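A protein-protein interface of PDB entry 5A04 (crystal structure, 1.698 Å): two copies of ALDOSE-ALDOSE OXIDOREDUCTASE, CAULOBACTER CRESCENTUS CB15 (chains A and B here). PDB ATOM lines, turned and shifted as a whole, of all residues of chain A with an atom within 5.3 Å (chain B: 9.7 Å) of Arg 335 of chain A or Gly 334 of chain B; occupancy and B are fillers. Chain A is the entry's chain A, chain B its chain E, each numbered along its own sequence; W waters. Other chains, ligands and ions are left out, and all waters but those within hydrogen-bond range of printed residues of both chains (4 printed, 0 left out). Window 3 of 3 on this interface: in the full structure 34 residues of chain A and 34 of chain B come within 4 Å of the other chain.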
ATOM      1  N   VAL A 205      15.951  27.716  -9.751  1.00  0.00           N
ATOM      2  CA  VAL A 205      17.301  28.132  -9.406  1.00  0.00           C
ATOM      3  C   VAL A 205      18.259  27.878 -10.566  1.00  0.00           C
ATOM      4  O   VAL A 205      18.278  26.772 -11.114  1.00  0.00           O
ATOM      5  CB  VAL A 205      17.817  27.350  -8.176  1.00  0.00           C
ATOM      6  CG1 VAL A 205      19.253  27.747  -7.855  1.00  0.00           C
ATOM      7  CG2 VAL A 205      16.895  27.563  -6.978  1.00  0.00           C
ATOM      8  N   ASN A 206      19.036  28.897 -10.935  1.00  0.00           N
ATOM      9  CA  ASN A 206      20.211  28.755 -11.812  1.00  0.00           C
ATOM     10  C   ASN A 206      21.460  29.050 -11.018  1.00  0.00           C
ATOM     11  O   ASN A 206      21.406  29.814 -10.055  1.00  0.00           O
ATOM     12  CB  ASN A 206      20.191  29.741 -12.996  1.00  0.00           C
ATOM     13  CG  ASN A 206      19.334  29.291 -14.146  1.00  0.00           C
ATOM     14  OD1 ASN A 206      19.084  28.097 -14.335  1.00  0.00           O
ATOM     15  ND2 ASN A 206      18.895  30.256 -14.955  1.00  0.00           N
ATOM     16  N   ARG A 329      23.472  21.971  -7.125  1.00  0.00           N
ATOM     17  CA  ARG A 329      23.062  21.045  -8.181  1.00  0.00           C
ATOM     18  C   ARG A 329      22.930  21.766  -9.520  1.00  0.00           C
ATOM     19  O   ARG A 329      23.344  21.240 -10.556  1.00  0.00           O
ATOM     20  CB  ARG A 329      21.747  20.356  -7.828  1.00  0.00           C
ATOM     21  CG  ARG A 329      21.253  19.390  -8.905  1.00  0.00           C
ATOM     22  CD  ARG A 329      20.102  18.541  -8.379  1.00  0.00           C
ATOM     23  NE  ARG A 329      20.467  17.893  -7.114  1.00  0.00           N
ATOM     24  CZ  ARG A 329      21.034  16.689  -7.004  1.00  0.00           C
ATOM     25  NH1 ARG A 329      21.299  15.972  -8.088  1.00  0.00           N
ATOM     26  NH2 ARG A 329      21.329  16.196  -5.805  1.00  0.00           N
ATOM     27  N   ALA A 330      22.385  22.981  -9.491  1.00  0.00           N
ATOM     28  CA  ALA A 330      22.200  23.751 -10.720  1.00  0.00           C
ATOM     29  C   ALA A 330      23.528  24.064 -11.381  1.00  0.00           C
ATOM     30  O   ALA A 330      23.627  24.030 -12.606  1.00  0.00           O
ATOM     31  CB  ALA A 330      21.426  25.052 -10.437  1.00  0.00           C
ATOM     32  N   GLU A 333      25.054  20.605 -12.680  1.00  0.00           N
ATOM     33  CA  GLU A 333      24.338  20.027 -13.824  1.00  0.00           C
ATOM     34  C   GLU A 333      24.135  20.991 -14.995  1.00  0.00           C
ATOM     35  O   GLU A 333      23.732  20.575 -16.086  1.00  0.00           O
ATOM     36  CB  GLU A 333      22.977  19.480 -13.359  1.00  0.00           C
ATOM     37  CG  GLU A 333      23.132  18.309 -12.370  1.00  0.00           C
ATOM     38  CD  GLU A 333      21.842  17.588 -12.021  1.00  0.00           C
ATOM     39  OE1 GLU A 333      20.787  17.887 -12.605  1.00  0.00           O
ATOM     40  OE2 GLU A 333      21.895  16.704 -11.147  1.00  0.00           O
ATOM     41  N   GLY A 334      24.412  22.270 -14.778  1.00  0.00           N
ATOM     42  CA  GLY A 334      24.197  23.281 -15.802  1.00  0.00           C
ATOM     43  C   GLY A 334      22.764  23.351 -16.304  1.00  0.00           C
ATOM     44  O   GLY A 334      22.508  23.401 -17.519  1.00  0.00           O
ATOM     45  N   ARG A 335      21.818  23.348 -15.376  1.00  0.00           N
ATOM     46  CA  ARG A 335      20.413  23.441 -15.743  1.00  0.00           C
ATOM     47  C   ARG A 335      19.623  24.115 -14.637  1.00  0.00           C
ATOM     48  O   ARG A 335      20.094  24.233 -13.504  1.00  0.00           O
ATOM     49  CB  ARG A 335      19.830  22.059 -16.046  1.00  0.00           C
ATOM     50  CG  ARG A 335      19.707  21.195 -14.835  1.00  0.00           C
ATOM     51  CD  ARG A 335      18.993  19.859 -15.101  1.00  0.00           C
ATOM     52  NE  ARG A 335      18.956  19.090 -13.855  1.00  0.00           N
ATOM     53  CZ  ARG A 335      17.996  19.186 -12.931  1.00  0.00           C
ATOM     54  NH1 ARG A 335      16.956  19.999 -13.112  1.00  0.00           N
ATOM     55  NH2 ARG A 335      18.068  18.455 -11.823  1.00  0.00           N
ATOM     56  N   THR A 336      18.433  24.589 -14.977  1.00  0.00           N
ATOM     57  CA  THR A 336      17.563  25.216 -13.992  1.00  0.00           C
ATOM     58  C   THR A 336      16.998  24.112 -13.106  1.00  0.00           C
ATOM     59  O   THR A 336      16.454  23.123 -13.608  1.00  0.00           O
ATOM     60  CB  THR A 336      16.440  26.020 -14.675  1.00  0.00           C
ATOM     61  OG1 THR A 336      17.032  26.968 -15.568  1.00  0.00           O
ATOM     62  CG2 THR A 336      15.592  26.769 -13.644  1.00  0.00           C
ATOM     63  N   VAL A 337      17.155  24.259 -11.796  1.00  0.00           N
ATOM     64  CA  VAL A 337      16.603  23.292 -10.861  1.00  0.00           C
ATOM     65  C   VAL A 337      15.290  23.803 -10.301  1.00  0.00           C
ATOM     66  O   VAL A 337      15.207  24.935  -9.808  1.00  0.00           O
ATOM     67  CB  VAL A 337      17.585  22.994  -9.711  1.00  0.00           C
ATOM     68  CG1 VAL A 337      16.918  22.114  -8.649  1.00  0.00           C
ATOM     69  CG2 VAL A 337      18.850  22.339 -10.267  1.00  0.00           C
ATOM     70  N   LYS A 338      14.254  22.968 -10.392  1.00  0.00           N
ATOM     71  CA  LYS A 338      12.932  23.350  -9.905  1.00  0.00           C
ATOM     72  C   LYS A 338      12.736  22.942  -8.451  1.00  0.00           C
ATOM     73  O   LYS A 338      13.159  21.865  -8.038  1.00  0.00           O
ATOM     74  CB  LYS A 338      11.842  22.716 -10.774  1.00  0.00           C
ATOM     75  CG  LYS A 338      11.770  23.279 -12.187  1.00  0.00           C
ATOM     76  CD  LYS A 338      10.526  22.766 -12.901  1.00  0.00           C
ATOM     77  CE  LYS A 338      10.422  23.300 -14.324  1.00  0.00           C
ATOM     78  NZ  LYS A 338       9.197  22.786 -15.003  1.00  0.00           N
ATOM     79  N   VAL B 205      26.175  30.695 -20.506  1.00  0.00           N
ATOM     80  CA  VAL B 205      25.085  31.626 -20.245  1.00  0.00           C
ATOM     81  C   VAL B 205      23.938  30.928 -19.516  1.00  0.00           C
ATOM     82  O   VAL B 205      23.488  29.872 -19.958  1.00  0.00           O
ATOM     83  CB  VAL B 205      24.533  32.227 -21.553  1.00  0.00           C
ATOM     84  CG1 VAL B 205      23.347  33.136 -21.264  1.00  0.00           C
ATOM     85  CG2 VAL B 205      25.630  32.975 -22.328  1.00  0.00           C
ATOM     86  N   ASN B 206      23.479  31.520 -18.409  1.00  0.00           N
ATOM     87  CA  ASN B 206      22.205  31.161 -17.764  1.00  0.00           C
ATOM     88  C   ASN B 206      21.234  32.310 -17.898  1.00  0.00           C
ATOM     89  O   ASN B 206      21.670  33.452 -17.974  1.00  0.00           O
ATOM     90  CB  ASN B 206      22.368  30.882 -16.262  1.00  0.00           C
ATOM     91  CG  ASN B 206      22.822  29.481 -15.967  1.00  0.00           C
ATOM     92  OD1 ASN B 206      22.594  28.554 -16.746  1.00  0.00           O
ATOM     93  ND2 ASN B 206      23.442  29.311 -14.813  1.00  0.00           N
ATOM     94  N   ALA B 207      19.935  32.032 -17.864  1.00  0.00           N
ATOM     95  CA  ALA B 207      18.948  33.117 -17.846  1.00  0.00           C
ATOM     96  C   ALA B 207      17.612  32.704 -17.249  1.00  0.00           C
ATOM     97  O   ALA B 207      17.225  31.537 -17.291  1.00  0.00           O
ATOM     98  CB  ALA B 207      18.735  33.666 -19.274  1.00  0.00           C
ATOM     99  N   VAL B 208      16.935  33.689 -16.669  1.00  0.00           N
ATOM    100  CA  VAL B 208      15.606  33.557 -16.085  1.00  0.00           C
ATOM    101  C   VAL B 208      14.749  34.683 -16.648  1.00  0.00           C
ATOM    102  O   VAL B 208      15.162  35.841 -16.607  1.00  0.00           O
ATOM    103  CB  VAL B 208      15.628  33.689 -14.536  1.00  0.00           C
ATOM    104  CG1 VAL B 208      14.212  33.785 -13.994  1.00  0.00           C
ATOM    105  CG2 VAL B 208      16.390  32.526 -13.885  1.00  0.00           C
ATOM    106  N   GLU B 209      13.566  34.358 -17.168  1.00  0.00           N
ATOM    107  CA  GLU B 209      12.630  35.381 -17.605  1.00  0.00           C
ATOM    108  C   GLU B 209      11.450  35.502 -16.657  1.00  0.00           C
ATOM    109  O   GLU B 209      10.980  34.510 -16.103  1.00  0.00           O
ATOM    110  CB  GLU B 209      12.091  35.092 -19.019  1.00  0.00           C
ATOM    111  CG  GLU B 209      11.100  36.183 -19.450  1.00  0.00           C
ATOM    112  CD  GLU B 209      10.225  35.823 -20.632  1.00  0.00           C
ATOM    113  OE1 GLU B 209      10.629  34.973 -21.461  1.00  0.00           O
ATOM    114  OE2 GLU B 209       9.129  36.419 -20.730  1.00  0.00           O
ATOM    115  N   GLN B 228      23.239  35.238 -16.444  1.00  0.00           N
ATOM    116  CA  GLN B 228      24.575  35.035 -15.903  1.00  0.00           C
ATOM    117  C   GLN B 228      25.540  34.709 -17.022  1.00  0.00           C
ATOM    118  O   GLN B 228      25.198  33.953 -17.928  1.00  0.00           O
ATOM    119  CB  GLN B 228      24.600  33.885 -14.895  1.00  0.00           C
ATOM    120  CG  GLN B 228      23.479  33.920 -13.870  1.00  0.00           C
ATOM    121  CD  GLN B 228      23.687  32.845 -12.819  1.00  0.00           C
ATOM    122  OE1 GLN B 228      23.447  31.670 -13.077  1.00  0.00           O
ATOM    123  NE2 GLN B 228      24.195  33.242 -11.639  1.00  0.00           N
ATOM    124  N   ALA B 326      21.771  33.405 -27.135  1.00  0.00           N
ATOM    125  CA  ALA B 326      22.041  32.396 -26.106  1.00  0.00           C
ATOM    126  C   ALA B 326      21.234  32.652 -24.835  1.00  0.00           C
ATOM    127  O   ALA B 326      20.764  31.721 -24.169  1.00  0.00           O
ATOM    128  CB  ALA B 326      23.528  32.369 -25.788  1.00  0.00           C
ATOM    129  N   ILE B 327      21.100  33.925 -24.485  1.00  0.00           N
ATOM    130  CA  ILE B 327      20.336  34.307 -23.308  1.00  0.00           C
ATOM    131  C   ILE B 327      18.864  33.921 -23.472  1.00  0.00           C
ATOM    132  O   ILE B 327      18.261  33.314 -22.582  1.00  0.00           O
ATOM    133  CB  ILE B 327      20.446  35.826 -23.041  1.00  0.00           C
ATOM    134  CG1 ILE B 327      21.858  36.194 -22.573  1.00  0.00           C
ATOM    135  CG2 ILE B 327      19.419  36.263 -21.996  1.00  0.00           C
ATOM    136  CD1 ILE B 327      22.168  37.704 -22.697  1.00  0.00           C
ATOM    137  N   TYR B 328      18.277  34.285 -24.610  1.00  0.00           N
ATOM    138  CA  TYR B 328      16.890  33.901 -24.867  1.00  0.00           C
ATOM    139  C   TYR B 328      16.731  32.382 -24.835  1.00  0.00           C
ATOM    140  O   TYR B 328      15.752  31.870 -24.286  1.00  0.00           O
ATOM    141  CB  TYR B 328      16.409  34.442 -26.213  1.00  0.00           C
ATOM    142  CG  TYR B 328      16.037  35.910 -26.201  1.00  0.00           C
ATOM    143  CD1 TYR B 328      15.208  36.442 -25.211  1.00  0.00           C
ATOM    144  CD2 TYR B 328      16.494  36.762 -27.201  1.00  0.00           C
ATOM    145  CE1 TYR B 328      14.856  37.795 -25.219  1.00  0.00           C
ATOM    146  CE2 TYR B 328      16.149  38.117 -27.210  1.00  0.00           C
ATOM    147  CZ  TYR B 328      15.330  38.621 -26.222  1.00  0.00           C
ATOM    148  OH  TYR B 328      14.977  39.961 -26.238  1.00  0.00           O
ATOM    149  N   ARG B 329      17.703  31.668 -25.400  1.00  0.00           N
ATOM    150  CA  ARG B 329      17.615  30.203 -25.445  1.00  0.00           C
ATOM    151  C   ARG B 329      17.739  29.605 -24.046  1.00  0.00           C
ATOM    152  O   ARG B 329      17.012  28.685 -23.692  1.00  0.00           O
ATOM    153  CB  ARG B 329      18.690  29.611 -26.359  1.00  0.00           C
ATOM    154  CG  ARG B 329      18.665  28.060 -26.412  1.00  0.00           C
ATOM    155  CD  ARG B 329      19.573  27.543 -27.534  1.00  0.00           C
ATOM    156  NE  ARG B 329      19.163  28.080 -28.834  1.00  0.00           N
ATOM    157  CZ  ARG B 329      18.157  27.592 -29.565  1.00  0.00           C
ATOM    158  NH1 ARG B 329      17.458  26.548 -29.126  1.00  0.00           N
ATOM    159  NH2 ARG B 329      17.846  28.145 -30.735  1.00  0.00           N
ATOM    160  N   ALA B 330      18.663  30.132 -23.251  1.00  0.00           N
ATOM    161  CA  ALA B 330      18.852  29.627 -21.892  1.00  0.00           C
ATOM    162  C   ALA B 330      17.599  29.795 -21.032  1.00  0.00           C
ATOM    163  O   ALA B 330      17.282  28.933 -20.209  1.00  0.00           O
ATOM    164  CB  ALA B 330      20.061  30.333 -21.229  1.00  0.00           C
ATOM    165  N   ALA B 331      16.893  30.908 -21.202  1.00  0.00           N
ATOM    166  CA  ALA B 331      15.671  31.139 -20.439  1.00  0.00           C
ATOM    167  C   ALA B 331      14.549  30.217 -20.920  1.00  0.00           C
ATOM    168  O   ALA B 331      13.730  29.739 -20.129  1.00  0.00           O
ATOM    169  CB  ALA B 331      15.246  32.597 -20.542  1.00  0.00           C
ATOM    170  N   ARG B 332      14.524  29.969 -22.226  1.00  0.00           N
ATOM    171  CA  ARG B 332      13.490  29.138 -22.822  1.00  0.00           C
ATOM    172  C   ARG B 332      13.676  27.672 -22.421  1.00  0.00           C
ATOM    173  O   ARG B 332      12.708  26.998 -22.064  1.00  0.00           O
ATOM    174  CB  ARG B 332      13.510  29.300 -24.354  1.00  0.00           C
ATOM    175  CG  ARG B 332      12.447  28.533 -25.130  1.00  0.00           C
ATOM    176  CD  ARG B 332      12.346  29.082 -26.578  1.00  0.00           C
ATOM    177  NE  ARG B 332      13.625  29.060 -27.299  1.00  0.00           N
ATOM    178  CZ  ARG B 332      14.264  30.144 -27.759  1.00  0.00           C
ATOM    179  NH1 ARG B 332      13.754  31.362 -27.591  1.00  0.00           N
ATOM    180  NH2 ARG B 332      15.420  30.013 -28.407  1.00  0.00           N
ATOM    181  N   GLU B 333      14.917  27.190 -22.463  1.00  0.00           N
ATOM    182  CA  GLU B 333      15.203  25.773 -22.250  1.00  0.00           C
ATOM    183  C   GLU B 333      15.561  25.421 -20.803  1.00  0.00           C
ATOM    184  O   GLU B 333      15.632  24.240 -20.450  1.00  0.00           O
ATOM    185  CB  GLU B 333      16.326  25.332 -23.193  1.00  0.00           C
ATOM    186  CG  GLU B 333      15.906  25.453 -24.662  1.00  0.00           C
ATOM    187  CD  GLU B 333      16.949  24.949 -25.638  1.00  0.00           C
ATOM    188  OE1 GLU B 333      18.008  24.470 -25.195  1.00  0.00           O
ATOM    189  OE2 GLU B 333      16.706  25.046 -26.863  1.00  0.00           O
ATOM    190  N   GLY B 334      15.774  26.442 -19.974  1.00  0.00           N
ATOM    191  CA  GLY B 334      16.131  26.229 -18.578  1.00  0.00           C
ATOM    192  C   GLY B 334      17.424  25.449 -18.426  1.00  0.00           C
ATOM    193  O   GLY B 334      17.509  24.476 -17.668  1.00  0.00           O
ATOM    194  N   ARG B 335      18.447  25.866 -19.160  1.00  0.00           N
ATOM    195  CA  ARG B 335      19.735  25.185 -19.085  1.00  0.00           C
ATOM    196  C   ARG B 335      20.852  26.172 -19.370  1.00  0.00           C
ATOM    197  O   ARG B 335      20.612  27.256 -19.905  1.00  0.00           O
ATOM    198  CB  ARG B 335      19.806  24.018 -20.071  1.00  0.00           C
ATOM    199  CG  ARG B 335      19.896  24.466 -21.506  1.00  0.00           C
ATOM    200  CD  ARG B 335      19.956  23.292 -22.477  1.00  0.00           C
ATOM    201  NE  ARG B 335      19.926  23.776 -23.852  1.00  0.00           N
ATOM    202  CZ  ARG B 335      21.011  24.067 -24.566  1.00  0.00           C
ATOM    203  NH1 ARG B 335      22.223  23.908 -24.036  1.00  0.00           N
ATOM    204  NH2 ARG B 335      20.880  24.516 -25.812  1.00  0.00           N
ATOM    205  N   THR B 336      22.067  25.794 -19.004  1.00  0.00           N
ATOM    206  CA  THR B 336      23.236  26.598 -19.314  1.00  0.00           C
ATOM    207  C   THR B 336      23.586  26.415 -20.774  1.00  0.00           C
ATOM    208  O   THR B 336      23.806  25.294 -21.228  1.00  0.00           O
ATOM    209  CB  THR B 336      24.429  26.205 -18.436  1.00  0.00           C
ATOM    210  OG1 THR B 336      24.031  26.257 -17.059  1.00  0.00           O
ATOM    211  CG2 THR B 336      25.599  27.157 -18.666  1.00  0.00           C
ATOM    212  N   VAL B 337      23.624  27.512 -21.514  1.00  0.00           N
ATOM    213  CA  VAL B 337      23.946  27.451 -22.936  1.00  0.00           C
ATOM    214  C   VAL B 337      25.428  27.735 -23.131  1.00  0.00           C
ATOM    215  O   VAL B 337      25.954  28.723 -22.609  1.00  0.00           O
ATOM    216  CB  VAL B 337      23.105  28.454 -23.738  1.00  0.00           C
ATOM    217  CG1 VAL B 337      23.616  28.553 -25.185  1.00  0.00           C
ATOM    218  CG2 VAL B 337      21.640  28.069 -23.678  1.00  0.00           C
HETATM  219  O   HOH W   1      19.136  29.159 -17.852  1.00  0.00           O
HETATM  220  O   HOH W   2      20.548  26.747 -16.306  1.00  0.00           O
HETATM  221  O   HOH W   3      15.558  29.345 -16.400  1.00  0.00           O
HETATM  222  O   HOH W   4      22.379  26.553 -13.669  1.00  0.00           O
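The side-chain hydroxyl (OG1) of Thr 336 of chain A is in hydrogen-bond range of the side-chain amide oxygen (OD1) of Asn 206 of chain A, 2.6 Å away.
The backbone carbonyl oxygen (O) of Ala 330 of chain A is in hydrogen-bond range of the backbone NH (N) of Arg 335 of chain A (3.4 Å).
The side-chain carboxylate (OE1) of Glu 333 of chain A lies within salt-bridge range of the guanidinium group (NE) of Arg 335 of chain A (2.5 Å).
The backbone NH (N) of Gln 228 of chain B is in hydrogen-bond range of the backbone carbonyl oxygen (O) of Asn 206 of chain B (2.8 Å).
O of Ala 330 of chain B is in hydrogen-bond range of N of Arg 335 of chain B (3.4 Å).
The guanidinium group (NE) of Arg 335 of chain B lies within salt-bridge range of the side-chain carboxylate (OE1) of Glu 333 of chain B, 2.4 Å away.
Water W2 lies within hydrogen-bond range of OD1 of Asn 206 of chain B, OD1 of Asn 206 of chain A, N of Thr 336 of chain B and N of Thr 336 of chain A.
Water W3 bridges O of Ala 207 of chain B (2.9 Å) and OG1 of Thr 336 of chain A (2.9 Å).
Water W1 lies within hydrogen-bond range of N of Ala 207 of chain B, O of Ala 330 of chain B, ND2 of Asn 206 of chain A and O of Arg 335 of chain B.
Water W4 lies within hydrogen-bond range of O of Ala 330 of chain A (3.0 Å), ND2 of Asn 206 of chain B (3.2 Å) and O of Arg 335 of chain A (3.3 Å).
Asn 206 of chain B touches its own counterpart, Asn 206 of chain A.
Gly 334 of chain A touches Arg 335 of chain B, and with the chains exchanged Arg 335 of chain A touches Gly 334 of chain B.
Gly 334 of chain A touches Thr 336 of chain B, and with the chains exchanged Thr 336 of chain A touches Gly 334 of chain B.
Arg 335 of chain A touches its own counterpart, Arg 335 of chain B.
Positions printed for both chains: 205, 206, 329, 330, 333, 334, 335, 336 and 337.
Of the 9 pairs that touch across the chains among the printed residues, 6 have their exchanged pair printed and touching as well.
Arg 335 of chain A touches two residues of chain B.
Gly 334 of chain B touches just these residues of chain A: Arg 335 (3.6 Å) and Thr 336 (2.8 Å).
No residue of chain B comes within 4 Å of Ala 330 of chain A.
No residue of chain B comes within 4 Å of Glu 333 of chain A.
Printed residues of chain B within 4 Å of Gly 334 of chain A: Arg 335 and Thr 336.
Printed residues of chain B within 4 Å of Asn 206 of chain A: Asn 206, Ala 207, Val 208 and Gln 228.
Printed residues of chain A within 4 Å of Arg 335 of chain B: Gly 334 (3.7 Å) and Arg 335 (3.8 Å).
Of the printed residues of chain A, Ala 207 of chain B touches Asn 206.
Of the printed residues of chain A, Val 208 of chain B touches Asn 206.
Of the printed residues of chain A, Asn 206 of chain B touches Asn 206.
The nearest residue of chain B that does not touch Arg 335 of chain A is Thr 336 of chain B (4.02 Å).
Of the 18 printed residues of chain B, 7 touch a printed residue of chain A.
Hydrophobic or aromatic side chains of chain B that line the printed part of chain A: Val 208.
Printed residues of chain A that touch a printed residue of chain B: Asn 206, Gly 334, Arg 335 and Thr 336.
Among the printed residues, 9 pairs touch across the chains.
Among the printed residues, merely in contact across the chains: Asn 206 of chain A with Val 208 of chain B, Arg 335 of chain A with Gly 334 of chain B, Gly 334 of chain A with Arg 335 of chain B, Asn 206 of chain A with Asn 206 of chain B, Asn 206 of chain A with Gln 228 of chain B and Arg 335 of chain A with Arg 335 of chain B.
ND2 of Asn 206 of chain A is in hydrogen-bond range of O of Ala 207 of chain B, at 3.1 Å.
The backbone carbonyl oxygen (O) of Gly 334 of chain A sits at hydrogen-bond distance from the backbone NH (N) of Thr 336 of chain B (2.9 Å).
O of Gly 334 of chain B sits at hydrogen-bond distance from N of Thr 336 of chain A (2.8 Å).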
